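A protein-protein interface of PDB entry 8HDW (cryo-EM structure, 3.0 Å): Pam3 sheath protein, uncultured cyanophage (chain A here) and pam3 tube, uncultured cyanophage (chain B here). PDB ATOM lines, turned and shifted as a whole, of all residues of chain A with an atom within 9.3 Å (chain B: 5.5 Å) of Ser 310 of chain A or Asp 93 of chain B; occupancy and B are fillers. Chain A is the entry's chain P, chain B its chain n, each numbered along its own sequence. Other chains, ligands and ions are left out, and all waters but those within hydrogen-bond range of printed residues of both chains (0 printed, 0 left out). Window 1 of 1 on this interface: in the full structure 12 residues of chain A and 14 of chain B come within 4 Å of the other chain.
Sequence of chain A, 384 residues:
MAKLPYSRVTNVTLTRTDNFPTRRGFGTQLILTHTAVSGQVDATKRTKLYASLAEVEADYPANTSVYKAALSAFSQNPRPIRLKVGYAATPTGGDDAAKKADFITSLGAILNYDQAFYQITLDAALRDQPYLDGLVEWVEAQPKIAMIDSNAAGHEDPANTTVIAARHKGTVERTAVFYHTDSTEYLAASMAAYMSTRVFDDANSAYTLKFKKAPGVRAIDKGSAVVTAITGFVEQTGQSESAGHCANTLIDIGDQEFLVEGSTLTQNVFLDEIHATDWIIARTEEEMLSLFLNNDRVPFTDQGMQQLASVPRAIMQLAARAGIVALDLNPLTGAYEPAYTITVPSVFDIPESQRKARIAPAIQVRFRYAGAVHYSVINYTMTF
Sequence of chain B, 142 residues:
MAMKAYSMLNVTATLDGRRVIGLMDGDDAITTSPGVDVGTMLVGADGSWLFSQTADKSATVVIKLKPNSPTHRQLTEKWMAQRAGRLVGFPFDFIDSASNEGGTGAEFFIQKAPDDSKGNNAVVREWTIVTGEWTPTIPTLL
The side-chain carboxylate (OD2) of Asp 93 of chain B is in salt-bridge range of the guanidinium group (NH1) of Arg 313 of chain A.
O of Thr 104 of chain B lies close to OE1 of Gln 317 of chain A (3.3 Å).
The backbone carbonyl oxygen of Thr 12 of chain B is in hydrogen-bond range of the backbone NH of Ile 95 of chain B (3.1 Å).
The backbone carbonyl oxygen (O) of Asp 93 of chain B sits at hydrogen-bond distance from the backbone NH (N) of Thr 14 of chain B.
The side-chain hydroxyl (OG1) of Thr 104 of chain B is in hydrogen-bond range of the side-chain carboxylate (OD2) of Asp 93 of chain B, at 3.4 Å.
NH2 of Arg 313 of chain A lies within hydrogen-bond range of OE1 of Gln 306 of chain A (3.4 Å).
The backbone carbonyl oxygen of Gln 307 of chain A lies within hydrogen-bond range of the side-chain hydroxyl of Ser 310 of chain A (2.5 Å).
Gln 306 of chain A touches Thr 12 of chain B.
OE1 of Gln 306 of chain A touches CG2 of Ile 95 of chain B, 3.4 Å away.
CG of Asp 93 of chain B touches CB of Ser 310 of chain A, 3.97 Å away.
CD1 of Ile 95 of chain B touches NH2 of Arg 313 of chain A, 3.2 Å away.
Arg 313 of chain A touches Thr 104 of chain B (O to CG2, 3.9 Å).
Ser 310 of chain A touches one residue of chain B.
Asp 93 of chain B touches just these residues of chain A: Ser 310 and Arg 313.
No residue of chain A comes within 4 Å of Ala 13 of chain B.
No residue of chain A comes within 4 Å of Thr 14 of chain B.
No residue of chain A comes within 4 Å of Phe 92 of chain B.
Of the printed residues of chain B, Gln 317 of chain A touches Thr 104.
Of the printed residues of chain A, Thr 12 of chain B touches Gln 306 (3.6 Å).
Of the printed residues of chain A, Ile 95 of chain B touches Gln 306 and Arg 313.
Of the printed residues of chain A, Thr 104 of chain B touches Arg 313 and Gln 317.
Of the printed residues of chain B, Gln 306 of chain A touches Thr 12 and Ile 95.
Leu 308 of chain A touches none of the printed residues of chain B.
Gly 304 of chain A touches none of the printed residues of chain B.
The nearest residue of chain B that does not touch Ser 310 of chain A is Thr 14 of chain B (4.2 Å).
Of the 12 printed residues of chain B, 4 touch a printed residue of chain A.
Hydrophobic or aromatic side chains of chain B within 4 Å of the printed part of chain A: Ile 95.
Of the 25 printed residues of chain A, 4 touch a printed residue of chain B.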
ATOM      1  N   THR A 284     -13.445 -15.101  16.810  1.00  0.00           N
ATOM      2  CA  THR A 284     -14.152 -14.972  15.538  1.00  0.00           C
ATOM      3  C   THR A 284     -13.441 -13.996  14.610  1.00  0.00           C
ATOM      4  O   THR A 284     -13.398 -14.207  13.395  1.00  0.00           O
ATOM      5  CB  THR A 284     -15.595 -14.530  15.760  1.00  0.00           C
ATOM      6  OG1 THR A 284     -15.610 -13.297  16.482  1.00  0.00           O
ATOM      7  CG2 THR A 284     -16.350 -15.566  16.539  1.00  0.00           C
ATOM      8  N   GLU A 287     -10.447 -15.947  13.095  1.00  0.00           N
ATOM      9  CA  GLU A 287     -10.859 -16.927  12.096  1.00  0.00           C
ATOM     10  C   GLU A 287     -11.377 -16.253  10.829  1.00  0.00           C
ATOM     11  O   GLU A 287     -11.128 -16.740   9.719  1.00  0.00           O
ATOM     12  CB  GLU A 287     -11.904 -17.868  12.687  1.00  0.00           C
ATOM     13  CG  GLU A 287     -11.335 -18.853  13.692  1.00  0.00           C
ATOM     14  CD  GLU A 287     -10.529 -19.973  13.044  1.00  0.00           C
ATOM     15  OE1 GLU A 287     -10.943 -20.476  11.977  1.00  0.00           O
ATOM     16  OE2 GLU A 287      -9.481 -20.359  13.605  1.00  0.00           O
ATOM     17  N   MET A 288     -12.083 -15.128  10.959  1.00  0.00           N
ATOM     18  CA  MET A 288     -12.491 -14.392   9.768  1.00  0.00           C
ATOM     19  C   MET A 288     -11.284 -13.920   8.974  1.00  0.00           C
ATOM     20  O   MET A 288     -11.255 -14.052   7.746  1.00  0.00           O
ATOM     21  CB  MET A 288     -13.362 -13.195  10.141  1.00  0.00           C
ATOM     22  CG  MET A 288     -14.758 -13.540  10.603  1.00  0.00           C
ATOM     23  SD  MET A 288     -15.769 -14.275   9.313  1.00  0.00           S
ATOM     24  CE  MET A 288     -15.501 -13.101   8.003  1.00  0.00           C
ATOM     25  N   LEU A 291      -9.739 -16.679   7.123  1.00  0.00           N
ATOM     26  CA  LEU A 291     -10.515 -17.020   5.938  1.00  0.00           C
ATOM     27  C   LEU A 291     -10.258 -16.096   4.758  1.00  0.00           C
ATOM     28  O   LEU A 291     -10.300 -16.549   3.616  1.00  0.00           O
ATOM     29  CB  LEU A 291     -12.014 -16.998   6.257  1.00  0.00           C
ATOM     30  CG  LEU A 291     -12.999 -17.410   5.166  1.00  0.00           C
ATOM     31  CD1 LEU A 291     -13.080 -18.914   5.073  1.00  0.00           C
ATOM     32  CD2 LEU A 291     -14.365 -16.823   5.433  1.00  0.00           C
ATOM     33  N   ASN A 295      -8.414 -17.987   0.879  1.00  0.00           N
ATOM     34  CA  ASN A 295      -9.144 -18.008  -0.376  1.00  0.00           C
ATOM     35  C   ASN A 295      -8.574 -17.002  -1.361  1.00  0.00           C
ATOM     36  O   ASN A 295      -7.999 -15.982  -0.980  1.00  0.00           O
ATOM     37  CB  ASN A 295     -10.615 -17.694  -0.143  1.00  0.00           C
ATOM     38  CG  ASN A 295     -11.285 -18.720   0.702  1.00  0.00           C
ATOM     39  OD1 ASN A 295     -11.674 -19.780   0.220  1.00  0.00           O
ATOM     40  ND2 ASN A 295     -11.441 -18.413   1.979  1.00  0.00           N
ATOM     41  N   VAL A 298     -13.745 -14.140  -1.746  1.00  0.00           N
ATOM     42  CA  VAL A 298     -15.039 -14.530  -1.201  1.00  0.00           C
ATOM     43  C   VAL A 298     -16.108 -13.805  -2.016  1.00  0.00           C
ATOM     44  O   VAL A 298     -16.244 -12.580  -1.904  1.00  0.00           O
ATOM     45  CB  VAL A 298     -15.154 -14.208   0.293  1.00  0.00           C
ATOM     46  CG1 VAL A 298     -16.523 -14.591   0.814  1.00  0.00           C
ATOM     47  CG2 VAL A 298     -14.090 -14.949   1.065  1.00  0.00           C
ATOM     48  N   ASP A 302     -24.850 -15.951  -2.385  1.00  0.00           N
ATOM     49  CA  ASP A 302     -25.308 -16.732  -1.238  1.00  0.00           C
ATOM     50  C   ASP A 302     -24.275 -17.767  -0.812  1.00  0.00           C
ATOM     51  O   ASP A 302     -24.150 -18.071   0.381  1.00  0.00           O
ATOM     52  CB  ASP A 302     -26.633 -17.414  -1.561  1.00  0.00           C
ATOM     53  CG  ASP A 302     -27.787 -16.435  -1.654  1.00  0.00           C
ATOM     54  OD1 ASP A 302     -27.720 -15.364  -1.014  1.00  0.00           O
ATOM     55  OD2 ASP A 302     -28.769 -16.739  -2.362  1.00  0.00           O
ATOM     56  N   GLN A 303     -23.533 -18.322  -1.772  1.00  0.00           N
ATOM     57  CA  GLN A 303     -22.452 -19.244  -1.445  1.00  0.00           C
ATOM     58  C   GLN A 303     -21.392 -18.560  -0.594  1.00  0.00           C
ATOM     59  O   GLN A 303     -20.859 -19.151   0.350  1.00  0.00           O
ATOM     60  CB  GLN A 303     -21.836 -19.802  -2.728  1.00  0.00           C
ATOM     61  CG  GLN A 303     -22.554 -21.011  -3.291  1.00  0.00           C
ATOM     62  CD  GLN A 303     -23.905 -20.676  -3.876  1.00  0.00           C
ATOM     63  OE1 GLN A 303     -24.260 -19.507  -4.021  1.00  0.00           O
ATOM     64  NE2 GLN A 303     -24.665 -21.701  -4.225  1.00  0.00           N
ATOM     65  N   GLY A 304     -21.076 -17.305  -0.916  1.00  0.00           N
ATOM     66  CA  GLY A 304     -20.179 -16.533  -0.081  1.00  0.00           C
ATOM     67  C   GLY A 304     -20.707 -16.267   1.309  1.00  0.00           C
ATOM     68  O   GLY A 304     -19.934 -16.312   2.268  1.00  0.00           O
ATOM     69  N   MET A 305     -22.005 -15.993   1.441  1.00  0.00           N
ATOM     70  CA  MET A 305     -22.593 -15.793   2.761  1.00  0.00           C
ATOM     71  C   MET A 305     -22.494 -17.054   3.607  1.00  0.00           C
ATOM     72  O   MET A 305     -22.204 -16.985   4.804  1.00  0.00           O
ATOM     73  CB  MET A 305     -24.049 -15.350   2.635  1.00  0.00           C
ATOM     74  CG  MET A 305     -24.250 -14.085   1.841  1.00  0.00           C
ATOM     75  SD  MET A 305     -23.172 -12.732   2.359  1.00  0.00           S
ATOM     76  CE  MET A 305     -23.671 -12.506   4.065  1.00  0.00           C
ATOM     77  N   GLN A 306     -22.747 -18.218   3.010  1.00  0.00           N
ATOM     78  CA  GLN A 306     -22.587 -19.457   3.766  1.00  0.00           C
ATOM     79  C   GLN A 306     -21.127 -19.724   4.116  1.00  0.00           C
ATOM     80  O   GLN A 306     -20.827 -20.196   5.220  1.00  0.00           O
ATOM     81  CB  GLN A 306     -23.181 -20.626   2.987  1.00  0.00           C
ATOM     82  CG  GLN A 306     -24.693 -20.602   2.908  1.00  0.00           C
ATOM     83  CD  GLN A 306     -25.356 -20.868   4.241  1.00  0.00           C
ATOM     84  OE1 GLN A 306     -24.710 -21.281   5.198  1.00  0.00           O
ATOM     85  NE2 GLN A 306     -26.655 -20.638   4.307  1.00  0.00           N
ATOM     86  N   GLN A 307     -20.205 -19.414   3.204  1.00  0.00           N
ATOM     87  CA  GLN A 307     -18.788 -19.556   3.517  1.00  0.00           C
ATOM     88  C   GLN A 307     -18.390 -18.663   4.688  1.00  0.00           C
ATOM     89  O   GLN A 307     -17.614 -19.076   5.556  1.00  0.00           O
ATOM     90  CB  GLN A 307     -17.950 -19.238   2.281  1.00  0.00           C
ATOM     91  CG  GLN A 307     -16.483 -19.573   2.422  1.00  0.00           C
ATOM     92  CD  GLN A 307     -15.700 -19.369   1.142  1.00  0.00           C
ATOM     93  OE1 GLN A 307     -16.237 -18.932   0.130  1.00  0.00           O
ATOM     94  NE2 GLN A 307     -14.420 -19.689   1.185  1.00  0.00           N
ATOM     95  N   LEU A 308     -18.901 -17.431   4.724  1.00  0.00           N
ATOM     96  CA  LEU A 308     -18.632 -16.547   5.854  1.00  0.00           C
ATOM     97  C   LEU A 308     -19.253 -17.077   7.139  1.00  0.00           C
ATOM     98  O   LEU A 308     -18.614 -17.062   8.193  1.00  0.00           O
ATOM     99  CB  LEU A 308     -19.150 -15.138   5.570  1.00  0.00           C
ATOM    100  CG  LEU A 308     -18.464 -14.286   4.508  1.00  0.00           C
ATOM    101  CD1 LEU A 308     -19.159 -12.954   4.389  1.00  0.00           C
ATOM    102  CD2 LEU A 308     -17.001 -14.088   4.836  1.00  0.00           C
ATOM    103  N   ALA A 309     -20.500 -17.544   7.072  1.00  0.00           N
ATOM    104  CA  ALA A 309     -21.200 -17.996   8.267  1.00  0.00           C
ATOM    105  C   ALA A 309     -20.656 -19.309   8.801  1.00  0.00           C
ATOM    106  O   ALA A 309     -21.021 -19.708   9.911  1.00  0.00           O
ATOM    107  CB  ALA A 309     -22.691 -18.135   7.979  1.00  0.00           C
ATOM    108  N   SER A 310     -19.818 -20.003   8.032  1.00  0.00           N
ATOM    109  CA  SER A 310     -19.191 -21.215   8.546  1.00  0.00           C
ATOM    110  C   SER A 310     -18.282 -20.957   9.746  1.00  0.00           C
ATOM    111  O   SER A 310     -17.957 -21.905  10.465  1.00  0.00           O
ATOM    112  CB  SER A 310     -18.394 -21.907   7.444  1.00  0.00           C
ATOM    113  OG  SER A 310     -17.311 -21.108   7.008  1.00  0.00           O
ATOM    114  N   VAL A 311     -17.865 -19.715   9.976  1.00  0.00           N
ATOM    115  CA  VAL A 311     -16.908 -19.382  11.033  1.00  0.00           C
ATOM    116  C   VAL A 311     -17.581 -19.341  12.407  1.00  0.00           C
ATOM    117  O   VAL A 311     -17.109 -20.025  13.332  1.00  0.00           O
ATOM    118  CB  VAL A 311     -16.177 -18.064  10.711  1.00  0.00           C
ATOM    119  CG1 VAL A 311     -15.513 -17.493  11.947  1.00  0.00           C
ATOM    120  CG2 VAL A 311     -15.155 -18.284   9.621  1.00  0.00           C
ATOM    121  N   PRO A 312     -18.664 -18.575  12.610  1.00  0.00           N
ATOM    122  CA  PRO A 312     -19.341 -18.639  13.914  1.00  0.00           C
ATOM    123  C   PRO A 312     -19.847 -20.021  14.275  1.00  0.00           C
ATOM    124  O   PRO A 312     -19.922 -20.339  15.465  1.00  0.00           O
ATOM    125  CB  PRO A 312     -20.492 -17.635  13.768  1.00  0.00           C
ATOM    126  CG  PRO A 312     -20.628 -17.399  12.341  1.00  0.00           C
ATOM    127  CD  PRO A 312     -19.275 -17.536  11.764  1.00  0.00           C
ATOM    128  N   ARG A 313     -20.189 -20.859  13.296  1.00  0.00           N
ATOM    129  CA  ARG A 313     -20.625 -22.213  13.611  1.00  0.00           C
ATOM    130  C   ARG A 313     -19.542 -23.028  14.291  1.00  0.00           C
ATOM    131  O   ARG A 313     -19.840 -23.767  15.229  1.00  0.00           O
ATOM    132  CB  ARG A 313     -21.082 -22.939  12.353  1.00  0.00           C
ATOM    133  CG  ARG A 313     -22.418 -22.488  11.832  1.00  0.00           C
ATOM    134  CD  ARG A 313     -22.964 -23.449  10.804  1.00  0.00           C
ATOM    135  NE  ARG A 313     -24.160 -22.909  10.177  1.00  0.00           N
ATOM    136  CZ  ARG A 313     -24.210 -22.443   8.936  1.00  0.00           C
ATOM    137  NH1 ARG A 313     -23.131 -22.465   8.167  1.00  0.00           N
ATOM    138  NH2 ARG A 313     -25.346 -21.961   8.460  1.00  0.00           N
ATOM    139  N   ALA A 314     -18.300 -22.926  13.832  1.00  0.00           N
ATOM    140  CA  ALA A 314     -17.177 -23.576  14.488  1.00  0.00           C
ATOM    141  C   ALA A 314     -16.828 -22.935  15.818  1.00  0.00           C
ATOM    142  O   ALA A 314     -16.499 -23.647  16.774  1.00  0.00           O
ATOM    143  CB  ALA A 314     -15.946 -23.549  13.581  1.00  0.00           C
ATOM    144  N   ILE A 315     -16.908 -21.607  15.907  1.00  0.00           N
ATOM    145  CA  ILE A 315     -16.570 -20.948  17.164  1.00  0.00           C
ATOM    146  C   ILE A 315     -17.563 -21.323  18.257  1.00  0.00           C
ATOM    147  O   ILE A 315     -17.186 -21.473  19.423  1.00  0.00           O
ATOM    148  CB  ILE A 315     -16.481 -19.425  16.972  1.00  0.00           C
ATOM    149  CG1 ILE A 315     -15.444 -19.088  15.907  1.00  0.00           C
ATOM    150  CG2 ILE A 315     -16.103 -18.756  18.274  1.00  0.00           C
ATOM    151  CD1 ILE A 315     -14.096 -19.676  16.174  1.00  0.00           C
ATOM    152  N   MET A 316     -18.841 -21.477  17.912  1.00  0.00           N
ATOM    153  CA  MET A 316     -19.825 -21.827  18.931  1.00  0.00           C
ATOM    154  C   MET A 316     -19.625 -23.251  19.436  1.00  0.00           C
ATOM    155  O   MET A 316     -19.825 -23.528  20.623  1.00  0.00           O
ATOM    156  CB  MET A 316     -21.242 -21.638  18.397  1.00  0.00           C
ATOM    157  CG  MET A 316     -21.606 -20.201  18.094  1.00  0.00           C
ATOM    158  SD  MET A 316     -21.175 -19.032  19.394  1.00  0.00           S
ATOM    159  CE  MET A 316     -22.296 -19.530  20.680  1.00  0.00           C
ATOM    160  N   GLN A 317     -19.238 -24.171  18.554  1.00  0.00           N
ATOM    161  CA  GLN A 317     -18.934 -25.522  19.009  1.00  0.00           C
ATOM    162  C   GLN A 317     -17.687 -25.537  19.879  1.00  0.00           C
ATOM    163  O   GLN A 317     -17.602 -26.303  20.843  1.00  0.00           O
ATOM    164  CB  GLN A 317     -18.763 -26.466  17.823  1.00  0.00           C
ATOM    165  CG  GLN A 317     -18.852 -27.921  18.218  1.00  0.00           C
ATOM    166  CD  GLN A 317     -18.298 -28.852  17.176  1.00  0.00           C
ATOM    167  OE1 GLN A 317     -19.043 -29.516  16.467  1.00  0.00           O
ATOM    168  NE2 GLN A 317     -16.981 -28.922  17.089  1.00  0.00           N
ATOM    169  N   ILE A 342     -27.744 -19.810  14.424  1.00  0.00           N
ATOM    170  CA  ILE A 342     -27.044 -18.928  13.495  1.00  0.00           C
ATOM    171  C   ILE A 342     -27.923 -18.740  12.269  1.00  0.00           C
ATOM    172  O   ILE A 342     -28.245 -19.713  11.578  1.00  0.00           O
ATOM    173  CB  ILE A 342     -25.671 -19.497  13.107  1.00  0.00           C
ATOM    174  CG1 ILE A 342     -24.834 -19.718  14.363  1.00  0.00           C
ATOM    175  CG2 ILE A 342     -24.963 -18.585  12.137  1.00  0.00           C
ATOM    176  CD1 ILE A 342     -23.422 -20.025  14.103  1.00  0.00           C
ATOM    177  N   VAL A 344     -28.354 -16.767   8.594  1.00  0.00           N
ATOM    178  CA  VAL A 344     -27.590 -16.154   7.518  1.00  0.00           C
ATOM    179  C   VAL A 344     -28.545 -15.330   6.663  1.00  0.00           C
ATOM    180  O   VAL A 344     -29.604 -15.825   6.271  1.00  0.00           O
ATOM    181  CB  VAL A 344     -26.877 -17.213   6.661  1.00  0.00           C
ATOM    182  CG1 VAL A 344     -25.849 -16.577   5.751  1.00  0.00           C
ATOM    183  CG2 VAL A 344     -26.241 -18.256   7.552  1.00  0.00           C
ATOM    184  N   ILE A 363     -24.609 -11.061   9.892  1.00  0.00           N
ATOM    185  CA  ILE A 363     -25.006 -12.387  10.347  1.00  0.00           C
ATOM    186  C   ILE A 363     -25.325 -12.315  11.833  1.00  0.00           C
ATOM    187  O   ILE A 363     -24.580 -11.708  12.606  1.00  0.00           O
ATOM    188  CB  ILE A 363     -23.895 -13.412  10.058  1.00  0.00           C
ATOM    189  CG1 ILE A 363     -23.635 -13.496   8.557  1.00  0.00           C
ATOM    190  CG2 ILE A 363     -24.265 -14.774  10.603  1.00  0.00           C
ATOM    191  CD1 ILE A 363     -22.321 -14.133   8.199  1.00  0.00           C
ATOM    192  N   THR B  12     -23.409 -25.973  -0.149  1.00  0.00           N
ATOM    193  CA  THR B  12     -22.064 -25.433  -0.012  1.00  0.00           C
ATOM    194  C   THR B  12     -21.306 -26.208   1.053  1.00  0.00           C
ATOM    195  O   THR B  12     -21.834 -26.460   2.138  1.00  0.00           O
ATOM    196  CB  THR B  12     -22.106 -23.943   0.328  1.00  0.00           C
ATOM    197  OG1 THR B  12     -21.067 -23.630   1.261  1.00  0.00           O
ATOM    198  CG2 THR B  12     -23.451 -23.573   0.919  1.00  0.00           C
ATOM    199  N   ALA B  13     -20.074 -26.596   0.733  1.00  0.00           N
ATOM    200  CA  ALA B  13     -19.202 -27.324   1.640  1.00  0.00           C
ATOM    201  C   ALA B  13     -17.874 -26.594   1.744  1.00  0.00           C
ATOM    202  O   ALA B  13     -17.283 -26.223   0.729  1.00  0.00           O
ATOM    203  CB  ALA B  13     -18.981 -28.759   1.163  1.00  0.00           C
ATOM    204  N   THR B  14     -17.408 -26.390   2.971  1.00  0.00           N
ATOM    205  CA  THR B  14     -16.212 -25.606   3.240  1.00  0.00           C
ATOM    206  C   THR B  14     -15.220 -26.466   4.001  1.00  0.00           C
ATOM    207  O   THR B  14     -15.528 -26.947   5.092  1.00  0.00           O
ATOM    208  CB  THR B  14     -16.548 -24.348   4.048  1.00  0.00           C
ATOM    209  OG1 THR B  14     -17.777 -23.788   3.578  1.00  0.00           O
ATOM    210  CG2 THR B  14     -15.459 -23.314   3.896  1.00  0.00           C
ATOM    211  N   LEU B  15     -14.035 -26.656   3.436  1.00  0.00           N
ATOM    212  CA  LEU B  15     -13.001 -27.488   4.044  1.00  0.00           C
ATOM    213  C   LEU B  15     -11.786 -26.612   4.308  1.00  0.00           C
ATOM    214  O   LEU B  15     -11.109 -26.186   3.369  1.00  0.00           O
ATOM    215  CB  LEU B  15     -12.653 -28.676   3.154  1.00  0.00           C
ATOM    216  CG  LEU B  15     -11.882 -29.830   3.792  1.00  0.00           C
ATOM    217  CD1 LEU B  15     -12.279 -31.123   3.139  1.00  0.00           C
ATOM    218  CD2 LEU B  15     -10.393 -29.634   3.662  1.00  0.00           C
ATOM    219  N   PRO B  91     -11.078 -27.394  10.336  1.00  0.00           N
ATOM    220  CA  PRO B  91     -12.538 -27.566  10.364  1.00  0.00           C
ATOM    221  C   PRO B  91     -13.131 -27.963   9.017  1.00  0.00           C
ATOM    222  O   PRO B  91     -12.593 -27.641   7.957  1.00  0.00           O
ATOM    223  CB  PRO B  91     -13.032 -26.181  10.780  1.00  0.00           C
ATOM    224  CG  PRO B  91     -12.015 -25.271  10.202  1.00  0.00           C
ATOM    225  CD  PRO B  91     -10.702 -25.972  10.382  1.00  0.00           C
ATOM    226  N   PHE B  92     -14.261 -28.669   9.071  1.00  0.00           N
ATOM    227  CA  PHE B  92     -15.080 -28.965   7.903  1.00  0.00           C
ATOM    228  C   PHE B  92     -16.529 -28.625   8.212  1.00  0.00           C
ATOM    229  O   PHE B  92     -16.993 -28.819   9.335  1.00  0.00           O
ATOM    230  CB  PHE B  92     -14.973 -30.434   7.477  1.00  0.00           C
ATOM    231  CG  PHE B  92     -15.922 -30.819   6.373  1.00  0.00           C
ATOM    232  CD1 PHE B  92     -15.646 -30.495   5.062  1.00  0.00           C
ATOM    233  CD2 PHE B  92     -17.088 -31.504   6.652  1.00  0.00           C
ATOM    234  CE1 PHE B  92     -16.511 -30.845   4.056  1.00  0.00           C
ATOM    235  CE2 PHE B  92     -17.954 -31.853   5.649  1.00  0.00           C
ATOM    236  CZ  PHE B  92     -17.666 -31.526   4.352  1.00  0.00           C
ATOM    237  N   ASP B  93     -17.241 -28.130   7.207  1.00  0.00           N
ATOM    238  CA  ASP B  93     -18.600 -27.647   7.393  1.00  0.00           C
ATOM    239  C   ASP B  93     -19.329 -27.748   6.064  1.00  0.00           C
ATOM    240  O   ASP B  93     -18.747 -27.461   5.019  1.00  0.00           O
ATOM    241  CB  ASP B  93     -18.569 -26.206   7.912  1.00  0.00           C
ATOM    242  CG  ASP B  93     -19.926 -25.542   7.918  1.00  0.00           C
ATOM    243  OD1 ASP B  93     -20.473 -25.268   6.831  1.00  0.00           O
ATOM    244  OD2 ASP B  93     -20.440 -25.271   9.019  1.00  0.00           O
ATOM    245  N   PHE B  94     -20.591 -28.174   6.099  1.00  0.00           N
ATOM    246  CA  PHE B  94     -21.426 -28.114   4.907  1.00  0.00           C
ATOM    247  C   PHE B  94     -22.891 -28.043   5.303  1.00  0.00           C
ATOM    248  O   PHE B  94     -23.299 -28.523   6.360  1.00  0.00           O
ATOM    249  CB  PHE B  94     -21.154 -29.285   3.943  1.00  0.00           C
ATOM    250  CG  PHE B  94     -21.832 -30.577   4.297  1.00  0.00           C
ATOM    251  CD1 PHE B  94     -21.843 -31.058   5.589  1.00  0.00           C
ATOM    252  CD2 PHE B  94     -22.425 -31.333   3.307  1.00  0.00           C
ATOM    253  CE1 PHE B  94     -22.459 -32.252   5.885  1.00  0.00           C
ATOM    254  CE2 PHE B  94     -23.037 -32.523   3.599  1.00  0.00           C
ATOM    255  CZ  PHE B  94     -23.054 -32.983   4.888  1.00  0.00           C
ATOM    256  N   ILE B  95     -23.682 -27.421   4.432  1.00  0.00           N
ATOM    257  CA  ILE B  95     -25.065 -27.089   4.744  1.00  0.00           C
ATOM    258  C   ILE B  95     -25.838 -27.001   3.437  1.00  0.00           C
ATOM    259  O   ILE B  95     -25.259 -26.846   2.366  1.00  0.00           O
ATOM    260  CB  ILE B  95     -25.148 -25.766   5.546  1.00  0.00           C
ATOM    261  CG1 ILE B  95     -26.494 -25.647   6.263  1.00  0.00           C
ATOM    262  CG2 ILE B  95     -24.903 -24.579   4.636  1.00  0.00           C
ATOM    263  CD1 ILE B  95     -26.817 -24.261   6.727  1.00  0.00           C
ATOM    264  N   GLY B 103     -24.227 -29.763   9.150  1.00  0.00           N
ATOM    265  CA  GLY B 103     -23.519 -29.909  10.406  1.00  0.00           C
ATOM    266  C   GLY B 103     -22.132 -29.324  10.296  1.00  0.00           C
ATOM    267  O   GLY B 103     -21.666 -28.970   9.211  1.00  0.00           O
ATOM    268  N   THR B 104     -21.465 -29.235  11.442  1.00  0.00           N
ATOM    269  CA  THR B 104     -20.141 -28.642  11.495  1.00  0.00           C
ATOM    270  C   THR B 104     -19.250 -29.466  12.413  1.00  0.00           C
ATOM    271  O   THR B 104     -19.722 -30.169  13.306  1.00  0.00           O
ATOM    272  CB  THR B 104     -20.200 -27.185  11.971  1.00  0.00           C
ATOM    273  OG1 THR B 104     -18.917 -26.573  11.812  1.00  0.00           O
ATOM    274  CG2 THR B 104     -20.590 -27.119  13.421  1.00  0.00           C
ATOM    275  N   GLY B 105     -17.949 -29.378  12.166  1.00  0.00           N
ATOM    276  CA  GLY B 105     -16.968 -29.956  13.057  1.00  0.00           C
ATOM    277  C   GLY B 105     -15.688 -29.148  13.008  1.00  0.00           C
ATOM    278  O   GLY B 105     -15.107 -28.932  11.946  1.00  0.00           O
